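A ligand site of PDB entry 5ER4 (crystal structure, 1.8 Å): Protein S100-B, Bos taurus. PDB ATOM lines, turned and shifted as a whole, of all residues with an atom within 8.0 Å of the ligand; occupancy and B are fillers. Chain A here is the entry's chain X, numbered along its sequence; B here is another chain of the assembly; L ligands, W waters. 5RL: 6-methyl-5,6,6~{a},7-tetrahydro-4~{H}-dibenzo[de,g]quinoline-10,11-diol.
NE2 of His 86 is in hydrogen-bond range of NE2 of His 16 of chain B.
Phe 89 touches the ligand.
Ile 12 of chain B touches the ligand.
Within 4 Å of the ligand: Cys 85, His 86, Phe 89, Ile 12 of chain B and Asp 13 of chain B.
The backbone carbonyl oxygen of His 86 sits at hydrogen-bond distance from an oxygen (O02) of the ligand (3.0 Å).
The backbone carbonyl oxygen (O) of Cys 85 lies within hydrogen-bond range of an oxygen (O02) of the ligand, at 2.6 Å.
N03 of the ligand lies within salt-bridge range of OD1 of Asp 13 of chain B, at 2.8 Å.
Water W1 lies within hydrogen-bond range of O01 of the ligand, O of His 86 and OE2 of Glu 90.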
ATOM      1  N   PHE A  44       9.580   5.124 -19.349  1.00  0.00           N
ATOM      2  CA  PHE A  44      10.863   4.601 -19.814  1.00  0.00           C
ATOM      3  C   PHE A  44      11.445   5.499 -20.890  1.00  0.00           C
ATOM      4  O   PHE A  44      12.631   5.845 -20.859  1.00  0.00           O
ATOM      5  CB  PHE A  44      10.684   3.197 -20.409  1.00  0.00           C
ATOM      6  CG  PHE A  44      10.413   2.108 -19.397  1.00  0.00           C
ATOM      7  CD1 PHE A  44      10.097   0.824 -19.822  1.00  0.00           C
ATOM      8  CD2 PHE A  44      10.498   2.355 -18.027  1.00  0.00           C
ATOM      9  CE1 PHE A  44       9.855  -0.198 -18.915  1.00  0.00           C
ATOM     10  CE2 PHE A  44      10.256   1.317 -17.105  1.00  0.00           C
ATOM     11  CZ  PHE A  44       9.930   0.053 -17.555  1.00  0.00           C
ATOM     12  N   THR A  82      13.608  -3.561 -23.646  1.00  0.00           N
ATOM     13  CA  THR A  82      13.932  -4.378 -22.481  1.00  0.00           C
ATOM     14  C   THR A  82      15.423  -4.387 -22.207  1.00  0.00           C
ATOM     15  O   THR A  82      15.855  -4.299 -21.062  1.00  0.00           O
ATOM     16  CB  THR A  82      13.411  -5.817 -22.648  1.00  0.00           C
ATOM     17  OG1 THR A  82      12.028  -5.783 -22.980  1.00  0.00           O
ATOM     18  CG2 THR A  82      13.612  -6.626 -21.364  1.00  0.00           C
ATOM     19  N   THR A  83      16.225  -4.493 -23.266  1.00  0.00           N
ATOM     20  CA  THR A  83      17.673  -4.442 -23.129  1.00  0.00           C
ATOM     21  C   THR A  83      18.126  -3.072 -22.603  1.00  0.00           C
ATOM     22  O   THR A  83      19.018  -2.977 -21.743  1.00  0.00           O
ATOM     23  CB  THR A  83      18.366  -4.761 -24.456  1.00  0.00           C
ATOM     24  OG1 THR A  83      17.952  -6.069 -24.880  1.00  0.00           O
ATOM     25  CG2 THR A  83      19.870  -4.757 -24.291  1.00  0.00           C
ATOM     26  N   ALA A  84      17.506  -2.013 -23.106  1.00  0.00           N
ATOM     27  CA  ALA A  84      17.854  -0.674 -22.662  1.00  0.00           C
ATOM     28  C   ALA A  84      17.426  -0.489 -21.212  1.00  0.00           C
ATOM     29  O   ALA A  84      18.135   0.147 -20.416  1.00  0.00           O
ATOM     30  CB  ALA A  84      17.197   0.368 -23.548  1.00  0.00           C
ATOM     31  N   CYS A  85      16.266  -1.035 -20.866  1.00  0.00           N
ATOM     32  CA  CYS A  85      15.781  -0.991 -19.495  1.00  0.00           C
ATOM     33  C   CYS A  85      16.751  -1.731 -18.590  1.00  0.00           C
ATOM     34  O   CYS A  85      17.059  -1.288 -17.483  1.00  0.00           O
ATOM     35  CB  CYS A  85      14.391  -1.636 -19.403  1.00  0.00           C
ATOM     36  SG  CYS A  85      13.551  -1.460 -17.811  1.00  0.00           S
ATOM     37  N   HIS A  86      17.248  -2.866 -19.081  1.00  0.00           N
ATOM     38  CA  HIS A  86      18.160  -3.704 -18.314  1.00  0.00           C
ATOM     39  C   HIS A  86      19.540  -3.055 -18.139  1.00  0.00           C
ATOM     40  O   HIS A  86      20.203  -3.256 -17.125  1.00  0.00           O
ATOM     41  CB  HIS A  86      18.316  -5.044 -19.019  1.00  0.00           C
ATOM     42  CG  HIS A  86      19.025  -6.073 -18.197  1.00  0.00           C
ATOM     43  ND1 HIS A  86      19.852  -7.022 -18.755  1.00  0.00           N
ATOM     44  CD2 HIS A  86      19.021  -6.320 -16.867  1.00  0.00           C
ATOM     45  CE1 HIS A  86      20.332  -7.799 -17.807  1.00  0.00           C
ATOM     46  NE2 HIS A  86      19.843  -7.390 -16.652  1.00  0.00           N
ATOM     47  N   GLU A  87      19.965  -2.289 -19.144  1.00  0.00           N
ATOM     48  CA  GLU A  87      21.310  -1.706 -19.133  1.00  0.00           C
ATOM     49  C   GLU A  87      21.368  -0.342 -18.450  1.00  0.00           C
ATOM     50  O   GLU A  87      22.451   0.182 -18.177  1.00  0.00           O
ATOM     51  CB  GLU A  87      21.867  -1.619 -20.555  1.00  0.00           C
ATOM     52  CG  GLU A  87      22.291  -2.970 -21.127  1.00  0.00           C
ATOM     53  CD  GLU A  87      22.720  -2.875 -22.578  1.00  0.00           C
ATOM     54  OE1 GLU A  87      23.355  -3.843 -23.071  1.00  0.00           O
ATOM     55  OE2 GLU A  87      22.412  -1.847 -23.224  1.00  0.00           O
ATOM     56  N   PHE A  88      20.196   0.217 -18.173  1.00  0.00           N
ATOM     57  CA  PHE A  88      20.118   1.571 -17.628  1.00  0.00           C
ATOM     58  C   PHE A  88      20.816   1.724 -16.283  1.00  0.00           C
ATOM     59  O   PHE A  88      21.401   2.767 -15.991  1.00  0.00           O
ATOM     60  CB  PHE A  88      18.661   2.015 -17.493  1.00  0.00           C
ATOM     61  CG  PHE A  88      18.513   3.459 -17.098  1.00  0.00           C
ATOM     62  CD1 PHE A  88      18.492   4.449 -18.062  1.00  0.00           C
ATOM     63  CD2 PHE A  88      18.396   3.816 -15.755  1.00  0.00           C
ATOM     64  CE1 PHE A  88      18.360   5.789 -17.704  1.00  0.00           C
ATOM     65  CE2 PHE A  88      18.258   5.157 -15.389  1.00  0.00           C
ATOM     66  CZ  PHE A  88      18.242   6.140 -16.374  1.00  0.00           C
ATOM     67  N   PHE A  89      20.751   0.682 -15.462  1.00  0.00           N
ATOM     68  CA  PHE A  89      21.240   0.744 -14.094  1.00  0.00           C
ATOM     69  C   PHE A  89      22.659   0.212 -13.934  1.00  0.00           C
ATOM     70  O   PHE A  89      23.115  -0.006 -12.814  1.00  0.00           O
ATOM     71  CB  PHE A  89      20.294   0.009 -13.149  1.00  0.00           C
ATOM     72  CG  PHE A  89      19.057   0.787 -12.801  1.00  0.00           C
ATOM     73  CD1 PHE A  89      19.119   2.146 -12.533  1.00  0.00           C
ATOM     74  CD2 PHE A  89      17.813   0.155 -12.747  1.00  0.00           C
ATOM     75  CE1 PHE A  89      17.980   2.855 -12.212  1.00  0.00           C
ATOM     76  CE2 PHE A  89      16.674   0.864 -12.426  1.00  0.00           C
ATOM     77  CZ  PHE A  89      16.753   2.219 -12.157  1.00  0.00           C
ATOM     78  N   GLU A  90      23.349  -0.013 -15.055  1.00  0.00           N
ATOM     79  CA  GLU A  90      24.735  -0.472 -15.038  1.00  0.00           C
ATOM     80  C   GLU A  90      25.703   0.685 -15.268  1.00  0.00           C
ATOM     81  O   GLU A  90      26.875   0.629 -14.860  1.00  0.00           O
ATOM     82  CB  GLU A  90      24.968  -1.577 -16.080  1.00  0.00           C
ATOM     83  CG  GLU A  90      23.955  -2.719 -16.059  1.00  0.00           C
ATOM     84  CD  GLU A  90      24.116  -3.656 -14.868  1.00  0.00           C
ATOM     85  OE1 GLU A  90      25.036  -4.497 -14.894  1.00  0.00           O
ATOM     86  OE2 GLU A  90      23.335  -3.548 -13.898  1.00  0.00           O
ATOM     87  N   MET B   1       2.877   2.042 -13.652  1.00  0.00           N
ATOM     88  CA  MET B   1       3.409   1.519 -14.912  1.00  0.00           C
ATOM     89  C   MET B   1       2.287   0.989 -15.794  1.00  0.00           C
ATOM     90  O   MET B   1       1.271   0.493 -15.282  1.00  0.00           O
ATOM     91  CB  MET B   1       4.408   0.389 -14.645  1.00  0.00           C
ATOM     92  CG  MET B   1       5.804   0.845 -14.245  1.00  0.00           C
ATOM     93  SD  MET B   1       7.010  -0.496 -14.351  1.00  0.00           S
ATOM     94  CE  MET B   1       6.522  -1.513 -12.954  1.00  0.00           C
ATOM     95  N   VAL B   8       7.789  -5.679 -19.504  1.00  0.00           N
ATOM     96  CA  VAL B   8       9.224  -5.523 -19.708  1.00  0.00           C
ATOM     97  C   VAL B   8      10.003  -5.850 -18.434  1.00  0.00           C
ATOM     98  O   VAL B   8      10.992  -6.577 -18.472  1.00  0.00           O
ATOM     99  CB  VAL B   8       9.590  -4.105 -20.191  1.00  0.00           C
ATOM    100  CG1 VAL B   8      11.092  -3.875 -20.088  1.00  0.00           C
ATOM    101  CG2 VAL B   8       9.122  -3.896 -21.620  1.00  0.00           C
ATOM    102  N   VAL B   9       9.529  -5.310 -17.311  1.00  0.00           N
ATOM    103  CA  VAL B   9      10.168  -5.555 -16.023  1.00  0.00           C
ATOM    104  C   VAL B   9      10.025  -7.014 -15.610  1.00  0.00           C
ATOM    105  O   VAL B   9      10.950  -7.589 -15.041  1.00  0.00           O
ATOM    106  CB  VAL B   9       9.601  -4.611 -14.932  1.00  0.00           C
ATOM    107  CG1 VAL B   9      10.251  -4.902 -13.575  1.00  0.00           C
ATOM    108  CG2 VAL B   9       9.824  -3.161 -15.329  1.00  0.00           C
ATOM    109  N   ALA B  10       8.897  -7.625 -15.933  1.00  0.00           N
ATOM    110  CA  ALA B  10       8.694  -9.057 -15.640  1.00  0.00           C
ATOM    111  C   ALA B  10       9.678  -9.953 -16.390  1.00  0.00           C
ATOM    112  O   ALA B  10      10.143 -10.972 -15.850  1.00  0.00           O
ATOM    113  CB  ALA B  10       7.257  -9.474 -15.923  1.00  0.00           C
ATOM    114  N   ILE B  12      12.757  -9.061 -17.299  1.00  0.00           N
ATOM    115  CA  ILE B  12      14.020  -8.889 -16.574  1.00  0.00           C
ATOM    116  C   ILE B  12      13.992  -9.694 -15.272  1.00  0.00           C
ATOM    117  O   ILE B  12      14.954 -10.412 -14.967  1.00  0.00           O
ATOM    118  CB  ILE B  12      14.318  -7.408 -16.338  1.00  0.00           C
ATOM    119  CG1 ILE B  12      14.571  -6.713 -17.684  1.00  0.00           C
ATOM    120  CG2 ILE B  12      15.541  -7.239 -15.436  1.00  0.00           C
ATOM    121  CD1 ILE B  12      14.573  -5.187 -17.635  1.00  0.00           C
ATOM    122  N   ASP B  13      12.884  -9.616 -14.530  1.00  0.00           N
ATOM    123  CA  ASP B  13      12.780 -10.283 -13.220  1.00  0.00           C
ATOM    124  C   ASP B  13      12.904 -11.788 -13.325  1.00  0.00           C
ATOM    125  O   ASP B  13      13.645 -12.408 -12.576  1.00  0.00           O
ATOM    126  CB  ASP B  13      11.483  -9.924 -12.494  1.00  0.00           C
ATOM    127  CG  ASP B  13      11.564  -8.608 -11.758  1.00  0.00           C
ATOM    128  OD1 ASP B  13      12.675  -8.089 -11.618  1.00  0.00           O
ATOM    129  OD2 ASP B  13      10.517  -8.089 -11.319  1.00  0.00           O
ATOM    130  N   VAL B  14      12.151 -12.387 -14.255  1.00  0.00           N
ATOM    131  CA  VAL B  14      12.205 -13.849 -14.386  1.00  0.00           C
ATOM    132  C   VAL B  14      13.586 -14.342 -14.839  1.00  0.00           C
ATOM    133  O   VAL B  14      14.057 -15.385 -14.383  1.00  0.00           O
ATOM    134  CB  VAL B  14      11.064 -14.424 -15.276  1.00  0.00           C
ATOM    135  CG1 VAL B  14      11.338 -14.128 -16.769  1.00  0.00           C
ATOM    136  CG2 VAL B  14      10.903 -15.921 -15.056  1.00  0.00           C
ATOM    137  N   PHE B  15      14.252 -13.594 -15.705  1.00  0.00           N
ATOM    138  CA  PHE B  15      15.575 -13.997 -16.168  1.00  0.00           C
ATOM    139  C   PHE B  15      16.547 -14.097 -14.990  1.00  0.00           C
ATOM    140  O   PHE B  15      17.269 -15.091 -14.830  1.00  0.00           O
ATOM    141  CB  PHE B  15      16.130 -12.986 -17.179  1.00  0.00           C
ATOM    142  CG  PHE B  15      17.536 -13.303 -17.625  1.00  0.00           C
ATOM    143  CD1 PHE B  15      17.763 -14.297 -18.571  1.00  0.00           C
ATOM    144  CD2 PHE B  15      18.620 -12.631 -17.085  1.00  0.00           C
ATOM    145  CE1 PHE B  15      19.053 -14.606 -18.983  1.00  0.00           C
ATOM    146  CE2 PHE B  15      19.928 -12.939 -17.482  1.00  0.00           C
ATOM    147  CZ  PHE B  15      20.138 -13.912 -18.446  1.00  0.00           C
ATOM    148  N   HIS B  16      16.554 -13.078 -14.154  1.00  0.00           N
ATOM    149  CA  HIS B  16      17.498 -13.003 -13.052  1.00  0.00           C
ATOM    150  C   HIS B  16      17.159 -13.958 -11.921  1.00  0.00           C
ATOM    151  O   HIS B  16      18.062 -14.482 -11.274  1.00  0.00           O
ATOM    152  CB  HIS B  16      17.604 -11.564 -12.549  1.00  0.00           C
ATOM    153  CG  HIS B  16      18.467 -10.717 -13.410  1.00  0.00           C
ATOM    154  ND1 HIS B  16      19.846 -10.765 -13.355  1.00  0.00           N
ATOM    155  CD2 HIS B  16      18.163  -9.811 -14.375  1.00  0.00           C
ATOM    156  CE1 HIS B  16      20.344  -9.918 -14.246  1.00  0.00           C
ATOM    157  NE2 HIS B  16      19.343  -9.325 -14.866  1.00  0.00           N
ATOM    158  N   GLN B  17      15.876 -14.187 -11.697  1.00  0.00           N
ATOM    159  CA  GLN B  17      15.437 -15.183 -10.723  1.00  0.00           C
ATOM    160  C   GLN B  17      16.096 -16.506 -10.998  1.00  0.00           C
ATOM    161  O   GLN B  17      16.539 -17.190 -10.069  1.00  0.00           O
ATOM    162  CB  GLN B  17      13.932 -15.366 -10.770  1.00  0.00           C
ATOM    163  CG  GLN B  17      13.167 -14.368  -9.931  1.00  0.00           C
ATOM    164  CD  GLN B  17      11.745 -14.216 -10.404  1.00  0.00           C
ATOM    165  OE1 GLN B  17      11.185 -15.128 -11.036  1.00  0.00           O
ATOM    166  NE2 GLN B  17      11.148 -13.056 -10.132  1.00  0.00           N
ATOM    167  N   HIS B  26      24.526 -14.047 -14.470  1.00  0.00           N
ATOM    168  CA  HIS B  26      23.934 -13.280 -15.549  1.00  0.00           C
ATOM    169  C   HIS B  26      23.677 -14.116 -16.791  1.00  0.00           C
ATOM    170  O   HIS B  26      23.369 -13.597 -17.859  1.00  0.00           O
ATOM    171  CB  HIS B  26      24.798 -12.057 -15.877  1.00  0.00           C
ATOM    172  CG  HIS B  26      25.014 -11.153 -14.705  1.00  0.00           C
ATOM    173  ND1 HIS B  26      24.173 -10.104 -14.422  1.00  0.00           N
ATOM    174  CD2 HIS B  26      25.954 -11.153 -13.739  1.00  0.00           C
ATOM    175  CE1 HIS B  26      24.598  -9.486 -13.335  1.00  0.00           C
ATOM    176  NE2 HIS B  26      25.671 -10.113 -12.898  1.00  0.00           N
ATOM    177  N   PHE B  71      21.409 -12.775 -21.551  1.00  0.00           N
ATOM    178  CA  PHE B  71      20.208 -11.958 -21.625  1.00  0.00           C
ATOM    179  C   PHE B  71      19.713 -11.762 -23.062  1.00  0.00           C
ATOM    180  O   PHE B  71      18.510 -11.835 -23.320  1.00  0.00           O
ATOM    181  CB  PHE B  71      20.386 -10.607 -20.919  1.00  0.00           C
ATOM    182  CG  PHE B  71      19.082  -9.869 -20.753  1.00  0.00           C
ATOM    183  CD1 PHE B  71      18.162 -10.274 -19.795  1.00  0.00           C
ATOM    184  CD2 PHE B  71      18.765  -8.795 -21.570  1.00  0.00           C
ATOM    185  CE1 PHE B  71      16.945  -9.611 -19.637  1.00  0.00           C
ATOM    186  CE2 PHE B  71      17.562  -8.112 -21.429  1.00  0.00           C
ATOM    187  CZ  PHE B  71      16.642  -8.533 -20.456  1.00  0.00           C
HETATM  188  C10 5RL L   1      16.645  -5.797 -11.968  1.00  0.00           C
HETATM  189  C11 5RL L   1      15.138  -4.176 -12.823  1.00  0.00           C
HETATM  190  C12 5RL L   1      16.408  -4.689 -12.828  1.00  0.00           C
HETATM  191  C13 5RL L   1      12.243  -5.254  -9.624  1.00  0.00           C
HETATM  192  C14 5RL L   1      17.100  -8.014 -10.236  1.00  0.00           C
HETATM  193  C15 5RL L   1      17.899  -6.391 -11.910  1.00  0.00           C
HETATM  194  C16 5RL L   1      14.755  -3.092 -13.617  1.00  0.00           C
HETATM  195  C19 5RL L   1      16.952  -2.982 -14.490  1.00  0.00           C
HETATM  196  C20 5RL L   1      15.676  -2.483 -14.461  1.00  0.00           C
HETATM  197  O01 5RL L   1      18.667  -4.391 -13.874  1.00  0.00           O
HETATM  198  O02 5RL L   1      17.905  -2.399 -15.316  1.00  0.00           O
HETATM  199  N03 5RL L   1      13.459  -5.969  -9.946  1.00  0.00           N
HETATM  200  C04 5RL L   1      14.292  -5.766 -11.116  1.00  0.00           C
HETATM  201  C05 5RL L   1      15.650  -6.348 -11.116  1.00  0.00           C
HETATM  202  C06 5RL L   1      14.010  -4.619 -12.032  1.00  0.00           C
HETATM  203  C07 5RL L   1      15.864  -7.386 -10.312  1.00  0.00           C
HETATM  204  C08 5RL L   1      13.820  -7.004  -8.953  1.00  0.00           C
HETATM  205  C09 5RL L   1      14.899  -8.041  -9.380  1.00  0.00           C
HETATM  206  C17 5RL L   1      17.344  -4.053 -13.702  1.00  0.00           C
HETATM  207  C18 5RL L   1      18.133  -7.490 -11.053  1.00  0.00           C
HETATM  208  O   HOH W   1      20.651  -3.185 -14.549  1.00  0.00           O
HETATM  209  O   HOH W   2      14.830 -11.188 -10.357  1.00  0.00           O
